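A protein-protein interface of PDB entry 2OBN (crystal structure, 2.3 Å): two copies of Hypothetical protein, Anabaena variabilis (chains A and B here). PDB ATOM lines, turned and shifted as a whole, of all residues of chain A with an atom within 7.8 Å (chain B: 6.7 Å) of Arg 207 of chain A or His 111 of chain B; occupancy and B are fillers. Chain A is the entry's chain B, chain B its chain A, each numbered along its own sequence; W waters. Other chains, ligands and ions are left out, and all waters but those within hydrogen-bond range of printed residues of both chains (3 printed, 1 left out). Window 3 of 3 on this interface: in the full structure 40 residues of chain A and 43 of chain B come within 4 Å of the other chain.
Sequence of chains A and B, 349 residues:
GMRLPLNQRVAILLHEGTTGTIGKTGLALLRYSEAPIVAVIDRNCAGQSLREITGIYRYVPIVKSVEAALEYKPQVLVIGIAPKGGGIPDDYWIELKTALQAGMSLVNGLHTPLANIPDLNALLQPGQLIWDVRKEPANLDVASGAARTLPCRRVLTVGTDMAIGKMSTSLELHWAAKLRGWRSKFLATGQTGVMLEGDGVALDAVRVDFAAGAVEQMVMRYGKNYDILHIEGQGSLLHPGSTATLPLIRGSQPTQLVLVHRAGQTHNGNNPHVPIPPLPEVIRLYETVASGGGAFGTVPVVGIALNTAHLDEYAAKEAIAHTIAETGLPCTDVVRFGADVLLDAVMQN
N of Val 208 of chain B touches O of Asp 204 of chain A, 3.5 Å away. Arg 207 of chain B touches Ala 205 of chain A. Arg 207 of chain B touches Val 206 of chain A. O of Asp 204 of chain B touches CB of Arg 207 of chain A, 3.8 Å away. O of Ala 205 of chain B touches CG of Arg 207 of chain A (3.5 Å). Arg 207 of chain A touches Val 206 of chain B. Leu 203 of chain B touches Val 208 of chain A (O to CB, 3.7 Å). His 111 of chain B touches Phe 210 of chain A. CB of Ala 211 of chain A touches CG2 of Val 208 of chain B, 3.6 Å away. CB of Pro 247 of chain A touches OG1 of Thr 243 of chain B, at 3.7 Å.
NH1 of Arg 134 of chain B sits close to NE2 of Gln 191 of chain B (3.2 Å). The side-chain carboxylate of Glu 136 of chain A lies within salt-bridge range of the guanidinium group of Arg 207 of chain A, 3.0 Å away. NE2 of His 111 of chain B lies close to NH2 of Arg 134 of chain B (3.5 Å). NH1 of Arg 134 of chain B lies within hydrogen-bond range of O of Gly 109 of chain B (2.8 Å). OE2 of Glu 136 of chain B is in salt-bridge range of NH2 of Arg 207 of chain B (3.1 Å). OD2 of Asp 204 of chain B is in salt-bridge range of NH2 of Arg 134 of chain B, at 3.0 Å.
Water W1 lies within hydrogen-bond range of the side-chain hydroxyl (OG1) of Thr 243 of chain B (2.6 Å), the backbone carbonyl oxygen (O) of Val 208 of chain A (2.8 Å) and the backbone NH (N) of Ala 212 of chain A (3.0 Å). Water W3 lies within hydrogen-bond range of ND1 of His 111 of chain B (2.8 Å) and NH1 of Arg 207 of chain A (3.0 Å). Water W2 bridges OD1 of Asp 209 of chain A (2.9 Å) and OD2 of Asp 204 of chain B (2.9 Å).
The backbone NH (N) of Val 208 of chain A is in hydrogen-bond range of the backbone carbonyl oxygen (O) of Asp 204 of chain B (3.4 Å). NE2 of His 111 of chain B lies within hydrogen-bond range of OD2 of Asp 209 of chain A, at 2.7 Å. The backbone NH of Val 208 of chain A is in hydrogen-bond range of the backbone carbonyl oxygen of Val 206 of chain B. OD2 of Asp 209 of chain A lies within salt-bridge range of NH2 of Arg 134 of chain B (3.7 Å). N of Val 208 of chain B is in hydrogen-bond range of O of Val 206 of chain A (2.8 Å). O of Asp 204 of chain B sits at hydrogen-bond distance from N of Asp 209 of chain A, 2.9 Å away.
Leu 203 of chain A touches Val 208 of chain B, and with the chains exchanged Val 208 of chain A touches Leu 203 of chain B. Asp 204 of chain A touches Arg 207 of chain B, and with the chains exchanged Arg 207 of chain A touches Asp 204 of chain B. Ala 205 of chain A touches Arg 207 of chain B, and with the chains exchanged Arg 207 of chain A touches Ala 205 of chain B. Val 206 of chain A touches Arg 207 of chain B, and with the chains exchanged Arg 207 of chain A touches Val 206 of chain B. 7 positions are printed for both chains.
Glu 136 of chain A touches none of the printed residues of chain B. Val 142 of chain A touches none of the printed residues of chain B. Of the printed residues of chain B, Val 206 of chain A touches Arg 207 (3.5 Å) and Val 208 (2.8 Å). Of chain B, only His 111, Asp 204, Ala 205 and Val 206 come within 4 Å of Arg 207 of chain A. Of the printed residues of chain B, Phe 210 of chain A touches His 111 (3.6 Å). Printed residues of chain A within 4 Å of His 111 of chain B: Arg 207 (3.6 Å), Asp 209 (2.7 Å) and Phe 210 (3.6 Å). Of the printed residues of chain A, Arg 134 of chain B touches Asp 209 (3.7 Å). Of the printed residues of chain A, Val 206 of chain B touches Arg 207 and Val 208. Printed residues of chain A within 4 Å of Thr 243 of chain B: Val 208 (3.8 Å) and Pro 247 (3.7 Å). The nearest residue of chain B that does not touch Arg 207 of chain A is Arg 207 of chain B (4.2 Å). The nearest printed residue of chain A that does not touch Thr 243 of chain B is Ala 211 of chain A (4.01 Å).
Hydrophobic or aromatic side chains of chain B within 4 Å of the printed part of chain A: His 111 and Val 208. Hydrophobic or aromatic side chains of chain A within 4 Å of the printed part of chain B: Val 208, Phe 210, Ala 211 and Pro 247. Among the printed residues, 20 pairs touch across the chains. Among the printed residues, Asp or Glu carboxylates within 4 Å of a Lys or Arg side-chain nitrogen of the other chain: Asp 209 of chain A with Arg 134 of chain B.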
ATOM      1  N   GLU A 136      -9.146   6.375  23.180  1.00  0.00           N
ATOM      2  CA  GLU A 136      -8.082   5.673  23.896  1.00  0.00           C
ATOM      3  C   GLU A 136      -7.042   6.638  24.468  1.00  0.00           C
ATOM      4  O   GLU A 136      -6.632   7.574  23.786  1.00  0.00           O
ATOM      5  CB  GLU A 136      -7.410   4.667  22.948  1.00  0.00           C
ATOM      6  CG  GLU A 136      -6.326   3.834  23.582  1.00  0.00           C
ATOM      7  CD  GLU A 136      -5.767   2.760  22.667  1.00  0.00           C
ATOM      8  OE1 GLU A 136      -6.546   2.038  22.002  1.00  0.00           O
ATOM      9  OE2 GLU A 136      -4.527   2.612  22.660  1.00  0.00           O
ATOM     10  N   PRO A 137      -6.618   6.431  25.726  1.00  0.00           N
ATOM     11  CA  PRO A 137      -5.559   7.311  26.230  1.00  0.00           C
ATOM     12  C   PRO A 137      -4.272   7.203  25.404  1.00  0.00           C
ATOM     13  O   PRO A 137      -4.003   6.172  24.772  1.00  0.00           O
ATOM     14  CB  PRO A 137      -5.310   6.795  27.649  1.00  0.00           C
ATOM     15  CG  PRO A 137      -6.524   6.023  28.011  1.00  0.00           C
ATOM     16  CD  PRO A 137      -7.044   5.451  26.738  1.00  0.00           C
ATOM     17  N   ALA A 138      -3.491   8.266  25.408  1.00  0.00           N
ATOM     18  CA  ALA A 138      -2.242   8.295  24.668  1.00  0.00           C
ATOM     19  C   ALA A 138      -1.099   7.606  25.417  1.00  0.00           C
ATOM     20  O   ALA A 138      -1.134   7.448  26.640  1.00  0.00           O
ATOM     21  CB  ALA A 138      -1.859   9.740  24.387  1.00  0.00           C
ATOM     22  N   ASN A 139      -0.080   7.229  24.652  1.00  0.00           N
ATOM     23  CA  ASN A 139       1.163   6.667  25.180  1.00  0.00           C
ATOM     24  C   ASN A 139       0.997   5.415  26.017  1.00  0.00           C
ATOM     25  O   ASN A 139       1.610   5.281  27.076  1.00  0.00           O
ATOM     26  CB  ASN A 139       1.924   7.738  25.987  1.00  0.00           C
ATOM     27  CG  ASN A 139       2.172   9.015  25.184  1.00  0.00           C
ATOM     28  OD1 ASN A 139       1.999  10.121  25.700  1.00  0.00           O
ATOM     29  ND2 ASN A 139       2.556   8.866  23.911  1.00  0.00           N
ATOM     30  N   LEU A 140       0.170   4.496  25.543  1.00  0.00           N
ATOM     31  CA  LEU A 140      -0.010   3.241  26.232  1.00  0.00           C
ATOM     32  C   LEU A 140       1.096   2.293  25.811  1.00  0.00           C
ATOM     33  O   LEU A 140       1.620   2.386  24.700  1.00  0.00           O
ATOM     34  CB  LEU A 140      -1.367   2.639  25.916  1.00  0.00           C
ATOM     35  CG  LEU A 140      -2.554   3.426  26.469  1.00  0.00           C
ATOM     36  CD1 LEU A 140      -3.843   2.708  26.106  1.00  0.00           C
ATOM     37  CD2 LEU A 140      -2.434   3.610  27.996  1.00  0.00           C
ATOM     38  N   VAL A 142       2.670  -1.993  26.779  1.00  0.00           N
ATOM     39  CA  VAL A 142       2.215  -3.294  27.240  1.00  0.00           C
ATOM     40  C   VAL A 142       2.447  -3.336  28.758  1.00  0.00           C
ATOM     41  O   VAL A 142       3.431  -2.783  29.255  1.00  0.00           O
ATOM     42  CB  VAL A 142       2.914  -4.438  26.469  1.00  0.00           C
ATOM     43  CG1 VAL A 142       2.500  -5.800  27.028  1.00  0.00           C
ATOM     44  CG2 VAL A 142       2.542  -4.348  24.981  1.00  0.00           C
ATOM     45  N   ALA A 202     -11.844   4.514  29.585  1.00  0.00           N
ATOM     46  CA  ALA A 202     -12.960   3.716  29.079  1.00  0.00           C
ATOM     47  C   ALA A 202     -12.328   2.469  28.457  1.00  0.00           C
ATOM     48  O   ALA A 202     -12.101   2.412  27.252  1.00  0.00           O
ATOM     49  CB  ALA A 202     -13.752   4.481  28.057  1.00  0.00           C
ATOM     50  N   LEU A 203     -12.047   1.482  29.300  1.00  0.00           N
ATOM     51  CA  LEU A 203     -11.324   0.275  28.894  1.00  0.00           C
ATOM     52  C   LEU A 203     -11.903  -0.515  27.731  1.00  0.00           C
ATOM     53  O   LEU A 203     -11.137  -1.065  26.943  1.00  0.00           O
ATOM     54  CB  LEU A 203     -11.173  -0.658  30.093  1.00  0.00           C
ATOM     55  CG  LEU A 203     -10.306  -1.900  29.917  1.00  0.00           C
ATOM     56  CD1 LEU A 203      -8.877  -1.507  29.608  1.00  0.00           C
ATOM     57  CD2 LEU A 203     -10.368  -2.764  31.169  1.00  0.00           C
ATOM     58  N   ASP A 204     -13.229  -0.557  27.582  1.00  0.00           N
ATOM     59  CA  ASP A 204     -13.826  -1.365  26.501  1.00  0.00           C
ATOM     60  C   ASP A 204     -13.596  -0.816  25.092  1.00  0.00           C
ATOM     61  O   ASP A 204     -13.878  -1.499  24.104  1.00  0.00           O
ATOM     62  CB  ASP A 204     -15.303  -1.692  26.758  1.00  0.00           C
ATOM     63  CG  ASP A 204     -16.239  -0.492  26.612  1.00  0.00           C
ATOM     64  OD1 ASP A 204     -15.833   0.602  26.201  1.00  0.00           O
ATOM     65  OD2 ASP A 204     -17.434  -0.673  26.917  1.00  0.00           O
ATOM     66  N   ALA A 205     -13.104   0.421  25.017  1.00  0.00           N
ATOM     67  CA  ALA A 205     -12.741   1.067  23.760  1.00  0.00           C
ATOM     68  C   ALA A 205     -11.228   1.051  23.525  1.00  0.00           C
ATOM     69  O   ALA A 205     -10.754   1.614  22.531  1.00  0.00           O
ATOM     70  CB  ALA A 205     -13.239   2.491  23.763  1.00  0.00           C
ATOM     71  N   VAL A 206     -10.461   0.461  24.449  1.00  0.00           N
ATOM     72  CA  VAL A 206      -9.005   0.361  24.285  1.00  0.00           C
ATOM     73  C   VAL A 206      -8.689  -0.882  23.443  1.00  0.00           C
ATOM     74  O   VAL A 206      -9.373  -1.915  23.552  1.00  0.00           O
ATOM     75  CB  VAL A 206      -8.272   0.268  25.647  1.00  0.00           C
ATOM     76  CG1 VAL A 206      -6.751   0.082  25.449  1.00  0.00           C
ATOM     77  CG2 VAL A 206      -8.537   1.515  26.486  1.00  0.00           C
ATOM     78  N   ARG A 207      -7.664  -0.784  22.593  1.00  0.00           N
ATOM     79  CA  ARG A 207      -7.254  -1.933  21.775  1.00  0.00           C
ATOM     80  C   ARG A 207      -6.749  -3.034  22.695  1.00  0.00           C
ATOM     81  O   ARG A 207      -6.128  -2.747  23.724  1.00  0.00           O
ATOM     82  CB  ARG A 207      -6.157  -1.542  20.779  1.00  0.00           C
ATOM     83  CG  ARG A 207      -6.634  -0.639  19.650  1.00  0.00           C
ATOM     84  CD  ARG A 207      -5.462  -0.043  18.892  1.00  0.00           C
ATOM     85  NE  ARG A 207      -4.804   1.020  19.650  1.00  0.00           N
ATOM     86  CZ  ARG A 207      -3.768   1.738  19.215  1.00  0.00           C
ATOM     87  NH1 ARG A 207      -3.221   1.509  18.033  1.00  0.00           N
ATOM     88  NH2 ARG A 207      -3.255   2.689  19.978  1.00  0.00           N
ATOM     89  N   VAL A 208      -7.000  -4.281  22.300  1.00  0.00           N
ATOM     90  CA  VAL A 208      -6.641  -5.459  23.106  1.00  0.00           C
ATOM     91  C   VAL A 208      -5.190  -5.427  23.610  1.00  0.00           C
ATOM     92  O   VAL A 208      -4.948  -5.595  24.810  1.00  0.00           O
ATOM     93  CB  VAL A 208      -6.987  -6.769  22.342  1.00  0.00           C
ATOM     94  CG1 VAL A 208      -6.262  -7.995  22.896  1.00  0.00           C
ATOM     95  CG2 VAL A 208      -8.488  -7.000  22.347  1.00  0.00           C
ATOM     96  N   ASP A 209      -4.259  -5.163  22.707  1.00  0.00           N
ATOM     97  CA  ASP A 209      -2.821  -5.135  23.004  1.00  0.00           C
ATOM     98  C   ASP A 209      -2.463  -4.188  24.165  1.00  0.00           C
ATOM     99  O   ASP A 209      -1.541  -4.462  24.946  1.00  0.00           O
ATOM    100  CB  ASP A 209      -2.047  -4.647  21.758  1.00  0.00           C
ATOM    101  CG  ASP A 209      -0.760  -5.406  21.495  1.00  0.00           C
ATOM    102  OD1 ASP A 209      -0.488  -6.439  22.136  1.00  0.00           O
ATOM    103  OD2 ASP A 209      -0.031  -4.995  20.569  1.00  0.00           O
ATOM    104  N   PHE A 210      -3.182  -3.072  24.269  1.00  0.00           N
ATOM    105  CA  PHE A 210      -2.870  -2.044  25.272  1.00  0.00           C
ATOM    106  C   PHE A 210      -3.820  -1.974  26.467  1.00  0.00           C
ATOM    107  O   PHE A 210      -3.651  -1.101  27.337  1.00  0.00           O
ATOM    108  CB  PHE A 210      -2.822  -0.687  24.581  1.00  0.00           C
ATOM    109  CG  PHE A 210      -1.829  -0.626  23.450  1.00  0.00           C
ATOM    110  CD1 PHE A 210      -0.463  -0.737  23.706  1.00  0.00           C
ATOM    111  CD2 PHE A 210      -2.251  -0.445  22.136  1.00  0.00           C
ATOM    112  CE1 PHE A 210       0.470  -0.671  22.681  1.00  0.00           C
ATOM    113  CE2 PHE A 210      -1.316  -0.357  21.096  1.00  0.00           C
ATOM    114  CZ  PHE A 210       0.048  -0.478  21.373  1.00  0.00           C
ATOM    115  N   ALA A 211      -4.775  -2.901  26.523  1.00  0.00           N
ATOM    116  CA  ALA A 211      -5.815  -2.897  27.545  1.00  0.00           C
ATOM    117  C   ALA A 211      -5.264  -3.008  28.960  1.00  0.00           C
ATOM    118  O   ALA A 211      -5.605  -2.196  29.821  1.00  0.00           O
ATOM    119  CB  ALA A 211      -6.856  -4.016  27.271  1.00  0.00           C
ATOM    120  N   ALA A 212      -4.422  -4.017  29.193  1.00  0.00           N
ATOM    121  CA  ALA A 212      -3.822  -4.212  30.505  1.00  0.00           C
ATOM    122  C   ALA A 212      -2.945  -3.020  30.864  1.00  0.00           C
ATOM    123  O   ALA A 212      -2.910  -2.587  32.022  1.00  0.00           O
ATOM    124  CB  ALA A 212      -3.006  -5.506  30.527  1.00  0.00           C
ATOM    125  N   GLY A 213      -2.254  -2.482  29.863  1.00  0.00           N
ATOM    126  CA  GLY A 213      -1.356  -1.328  30.033  1.00  0.00           C
ATOM    127  C   GLY A 213      -2.127  -0.076  30.412  1.00  0.00           C
ATOM    128  O   GLY A 213      -1.635   0.763  31.162  1.00  0.00           O
ATOM    129  N   ALA A 214      -3.356   0.032  29.904  1.00  0.00           N
ATOM    130  CA  ALA A 214      -4.216   1.166  30.211  1.00  0.00           C
ATOM    131  C   ALA A 214      -4.599   1.129  31.684  1.00  0.00           C
ATOM    132  O   ALA A 214      -4.683   2.155  32.332  1.00  0.00           O
ATOM    133  CB  ALA A 214      -5.485   1.135  29.326  1.00  0.00           C
ATOM    134  N   PRO A 247      -7.923  -7.814  31.445  1.00  0.00           N
ATOM    135  CA  PRO A 247      -6.988  -6.691  31.648  1.00  0.00           C
ATOM    136  C   PRO A 247      -7.161  -5.949  32.975  1.00  0.00           C
ATOM    137  O   PRO A 247      -6.185  -5.433  33.502  1.00  0.00           O
ATOM    138  CB  PRO A 247      -7.274  -5.761  30.455  1.00  0.00           C
ATOM    139  CG  PRO A 247      -8.599  -6.216  29.893  1.00  0.00           C
ATOM    140  CD  PRO A 247      -8.691  -7.663  30.193  1.00  0.00           C
ATOM    141  N   GLY B  86       5.943   2.414  21.240  1.00  0.00           N
ATOM    142  CA  GLY B  86       6.379   3.302  20.171  1.00  0.00           C
ATOM    143  C   GLY B  86       5.519   3.142  18.930  1.00  0.00           C
ATOM    144  O   GLY B  86       4.959   2.071  18.691  1.00  0.00           O
ATOM    145  N   GLY B  87       5.414   4.212  18.143  1.00  0.00           N
ATOM    146  CA  GLY B  87       4.620   4.217  16.914  1.00  0.00           C
ATOM    147  C   GLY B  87       5.496   3.936  15.708  1.00  0.00           C
ATOM    148  O   GLY B  87       5.912   2.792  15.483  1.00  0.00           O
ATOM    149  N   ASN B 108       1.792  -3.106   5.968  1.00  0.00           N
ATOM    150  CA  ASN B 108       2.040  -2.547   7.297  1.00  0.00           C
ATOM    151  C   ASN B 108       1.390  -3.325   8.439  1.00  0.00           C
ATOM    152  O   ASN B 108       0.173  -3.388   8.557  1.00  0.00           O
ATOM    153  CB  ASN B 108       1.578  -1.087   7.340  1.00  0.00           C
ATOM    154  CG  ASN B 108       1.757  -0.472   8.702  1.00  0.00           C
ATOM    155  OD1 ASN B 108       2.719  -0.772   9.405  1.00  0.00           O
ATOM    156  ND2 ASN B 108       0.838   0.397   9.083  1.00  0.00           N
ATOM    157  N   GLY B 109       2.230  -3.908   9.289  1.00  0.00           N
ATOM    158  CA  GLY B 109       1.771  -4.651  10.449  1.00  0.00           C
ATOM    159  C   GLY B 109       1.846  -3.871  11.752  1.00  0.00           C
ATOM    160  O   GLY B 109       1.577  -4.429  12.816  1.00  0.00           O
ATOM    161  N   LEU B 110       2.217  -2.599  11.684  1.00  0.00           N
ATOM    162  CA  LEU B 110       2.302  -1.768  12.872  1.00  0.00           C
ATOM    163  C   LEU B 110       0.905  -1.381  13.313  1.00  0.00           C
ATOM    164  O   LEU B 110      -0.053  -1.478  12.542  1.00  0.00           O
ATOM    165  CB  LEU B 110       3.069  -0.468  12.580  1.00  0.00           C
ATOM    166  CG  LEU B 110       4.539  -0.528  12.148  1.00  0.00           C
ATOM    167  CD1 LEU B 110       5.027   0.856  11.656  1.00  0.00           C
ATOM    168  CD2 LEU B 110       5.419  -1.041  13.270  1.00  0.00           C
ATOM    169  N   HIS B 111       0.802  -0.923  14.553  1.00  0.00           N
ATOM    170  CA  HIS B 111      -0.461  -0.421  15.082  1.00  0.00           C
ATOM    171  C   HIS B 111      -0.840   0.917  14.461  1.00  0.00           C
ATOM    172  O   HIS B 111      -2.021   1.251  14.381  1.00  0.00           O
ATOM    173  CB  HIS B 111      -0.407  -0.248  16.591  1.00  0.00           C
ATOM    174  CG  HIS B 111      -0.683  -1.497  17.356  1.00  0.00           C
ATOM    175  ND1 HIS B 111      -1.937  -2.064  17.401  1.00  0.00           N
ATOM    176  CD2 HIS B 111       0.099  -2.234  18.179  1.00  0.00           C
ATOM    177  CE1 HIS B 111      -1.907  -3.119  18.197  1.00  0.00           C
ATOM    178  NE2 HIS B 111      -0.686  -3.237  18.690  1.00  0.00           N
ATOM    179  N   THR B 112       0.162   1.691  14.058  1.00  0.00           N
ATOM    180  CA  THR B 112      -0.082   2.982  13.425  1.00  0.00           C
ATOM    181  C   THR B 112      -0.393   2.733  11.957  1.00  0.00           C
ATOM    182  O   THR B 112       0.443   2.155  11.253  1.00  0.00           O
ATOM    183  CB  THR B 112       1.131   3.922  13.515  1.00  0.00           C
ATOM    184  OG1 THR B 112       1.486   4.126  14.895  1.00  0.00           O
ATOM    185  CG2 THR B 112       0.795   5.273  12.866  1.00  0.00           C
ATOM    186  N   PRO B 113      -1.597   3.148  11.500  1.00  0.00           N
ATOM    187  CA  PRO B 113      -1.970   2.954  10.109  1.00  0.00           C
ATOM    188  C   PRO B 113      -1.269   3.955   9.216  1.00  0.00           C
ATOM    189  O   PRO B 113      -1.176   5.131   9.592  1.00  0.00           O
ATOM    190  CB  PRO B 113      -3.485   3.206  10.105  1.00  0.00           C
ATOM    191  CG  PRO B 113      -3.732   4.127  11.248  1.00  0.00           C
ATOM    192  CD  PRO B 113      -2.673   3.811  12.276  1.00  0.00           C
ATOM    193  N   ARG B 134      -3.418  -4.369  10.653  1.00  0.00           N
ATOM    194  CA  ARG B 134      -4.063  -4.219  11.958  1.00  0.00           C
ATOM    195  C   ARG B 134      -5.354  -3.390  12.015  1.00  0.00           C
ATOM    196  O   ARG B 134      -5.804  -3.051  13.078  1.00  0.00           O
ATOM    197  CB  ARG B 134      -3.049  -3.674  12.976  1.00  0.00           C
ATOM    198  CG  ARG B 134      -2.248  -4.771  13.620  1.00  0.00           C
ATOM    199  CD  ARG B 134      -1.221  -4.192  14.529  1.00  0.00           C
ATOM    200  NE  ARG B 134      -0.803  -5.110  15.583  1.00  0.00           N
ATOM    201  CZ  ARG B 134       0.423  -5.163  16.108  1.00  0.00           C
ATOM    202  NH1 ARG B 134       1.423  -4.439  15.629  1.00  0.00           N
ATOM    203  NH2 ARG B 134       0.675  -6.007  17.091  1.00  0.00           N
ATOM    204  N   GLU B 136      -9.038  -2.723  12.399  1.00  0.00           N
ATOM    205  CA  GLU B 136     -10.141  -3.469  12.969  1.00  0.00           C
ATOM    206  C   GLU B 136     -11.210  -3.670  11.874  1.00  0.00           C
ATOM    207  O   GLU B 136     -11.523  -2.726  11.143  1.00  0.00           O
ATOM    208  CB  GLU B 136     -10.735  -2.686  14.136  1.00  0.00           C
ATOM    209  CG  GLU B 136     -11.892  -3.379  14.803  1.00  0.00           C
ATOM    210  CD  GLU B 136     -12.483  -2.579  15.937  1.00  0.00           C
ATOM    211  OE1 GLU B 136     -11.722  -2.067  16.782  1.00  0.00           O
ATOM    212  OE2 GLU B 136     -13.724  -2.502  15.993  1.00  0.00           O
ATOM    213  N   GLN B 191      -1.214 -10.213  13.009  1.00  0.00           N
ATOM    214  CA  GLN B 191      -0.624  -9.647  11.783  1.00  0.00           C
ATOM    215  C   GLN B 191       0.160 -10.639  10.934  1.00  0.00           C
ATOM    216  O   GLN B 191       0.025 -10.637   9.711  1.00  0.00           O
ATOM    217  CB  GLN B 191       0.290  -8.455  12.113  1.00  0.00           C
ATOM    218  CG  GLN B 191       1.380  -8.761  13.137  1.00  0.00           C
ATOM    219  CD  GLN B 191       2.402  -7.661  13.261  1.00  0.00           C
ATOM    220  OE1 GLN B 191       2.991  -7.229  12.270  1.00  0.00           O
ATOM    221  NE2 GLN B 191       2.652  -7.226  14.496  1.00  0.00           N
ATOM    222  N   LEU B 203      -6.262  -9.541  15.983  1.00  0.00           N
ATOM    223  CA  LEU B 203      -7.022  -9.378  17.226  1.00  0.00           C
ATOM    224  C   LEU B 203      -6.543  -8.314  18.193  1.00  0.00           C
ATOM    225  O   LEU B 203      -7.365  -7.635  18.799  1.00  0.00           O
ATOM    226  CB  LEU B 203      -7.113 -10.711  17.978  1.00  0.00           C
ATOM    227  CG  LEU B 203      -8.115 -10.752  19.146  1.00  0.00           C
ATOM    228  CD1 LEU B 203      -9.485 -10.223  18.719  1.00  0.00           C
ATOM    229  CD2 LEU B 203      -8.208 -12.166  19.663  1.00  0.00           C
ATOM    230  N   ASP B 204      -5.229  -8.169  18.338  1.00  0.00           N
ATOM    231  CA  ASP B 204      -4.692  -7.227  19.297  1.00  0.00           C
ATOM    232  C   ASP B 204      -4.969  -5.755  18.983  1.00  0.00           C
ATOM    233  O   ASP B 204      -4.790  -4.906  19.841  1.00  0.00           O
ATOM    234  CB  ASP B 204      -3.202  -7.479  19.566  1.00  0.00           C
ATOM    235  CG  ASP B 204      -2.333  -7.332  18.344  1.00  0.00           C
ATOM    236  OD1 ASP B 204      -2.725  -6.664  17.358  1.00  0.00           O
ATOM    237  OD2 ASP B 204      -1.220  -7.910  18.389  1.00  0.00           O
ATOM    238  N   ALA B 205      -5.391  -5.468  17.757  1.00  0.00           N
ATOM    239  CA  ALA B 205      -5.760  -4.119  17.339  1.00  0.00           C
ATOM    240  C   ALA B 205      -7.273  -3.871  17.450  1.00  0.00           C
ATOM    241  O   ALA B 205      -7.751  -2.791  17.116  1.00  0.00           O
ATOM    242  CB  ALA B 205      -5.304  -3.890  15.912  1.00  0.00           C
ATOM    243  N   VAL B 206      -8.033  -4.864  17.906  1.00  0.00           N
ATOM    244  CA  VAL B 206      -9.471  -4.695  18.017  1.00  0.00           C
ATOM    245  C   VAL B 206      -9.786  -4.132  19.388  1.00  0.00           C
ATOM    246  O   VAL B 206      -9.144  -4.520  20.364  1.00  0.00           O
ATOM    247  CB  VAL B 206     -10.219  -6.035  17.828  1.00  0.00           C
ATOM    248  CG1 VAL B 206     -11.717  -5.848  17.981  1.00  0.00           C
ATOM    249  CG2 VAL B 206      -9.888  -6.659  16.471  1.00  0.00           C
ATOM    250  N   ARG B 207     -10.767  -3.223  19.459  1.00  0.00           N
ATOM    251  CA  ARG B 207     -11.246  -2.692  20.750  1.00  0.00           C
ATOM    252  C   ARG B 207     -11.772  -3.827  21.648  1.00  0.00           C
ATOM    253  O   ARG B 207     -12.443  -4.754  21.165  1.00  0.00           O
ATOM    254  CB  ARG B 207     -12.354  -1.668  20.542  1.00  0.00           C
ATOM    255  CG  ARG B 207     -11.871  -0.358  19.945  1.00  0.00           C
ATOM    256  CD  ARG B 207     -13.018   0.537  19.557  1.00  0.00           C
ATOM    257  NE  ARG B 207     -13.676   0.070  18.334  1.00  0.00           N
ATOM    258  CZ  ARG B 207     -14.738   0.635  17.764  1.00  0.00           C
ATOM    259  NH1 ARG B 207     -15.330   1.683  18.304  1.00  0.00           N
ATOM    260  NH2 ARG B 207     -15.232   0.123  16.645  1.00  0.00           N
ATOM    261  N   VAL B 208     -11.447  -3.752  22.943  1.00  0.00           N
ATOM    262  CA  VAL B 208     -11.834  -4.779  23.948  1.00  0.00           C
ATOM    263  C   VAL B 208     -13.311  -5.218  23.836  1.00  0.00           C
ATOM    264  O   VAL B 208     -13.616  -6.422  23.844  1.00  0.00           O
ATOM    265  CB  VAL B 208     -11.499  -4.276  25.399  1.00  0.00           C
ATOM    266  CG1 VAL B 208     -12.290  -5.014  26.471  1.00  0.00           C
ATOM    267  CG2 VAL B 208     -10.008  -4.378  25.670  1.00  0.00           C
ATOM    268  N   THR B 243      -4.034 -10.047  27.028  1.00  0.00           N
ATOM    269  CA  THR B 243      -5.503 -10.070  27.015  1.00  0.00           C
ATOM    270  C   THR B 243      -6.115 -11.019  25.972  1.00  0.00           C
ATOM    271  O   THR B 243      -7.152 -11.644  26.225  1.00  0.00           O
ATOM    272  CB  THR B 243      -6.017  -8.649  26.731  1.00  0.00           C
ATOM    273  OG1 THR B 243      -5.713  -7.812  27.849  1.00  0.00           O
ATOM    274  CG2 THR B 243      -7.510  -8.615  26.497  1.00  0.00           C
HETATM  275  O   HOH W   1      -3.792  -6.220  27.281  1.00  0.00           O
HETATM  276  O   HOH W   2       0.216  -8.830  20.734  1.00  0.00           O
HETATM  277  O   HOH W   3      -3.825  -0.602  16.006  1.00  0.00           O
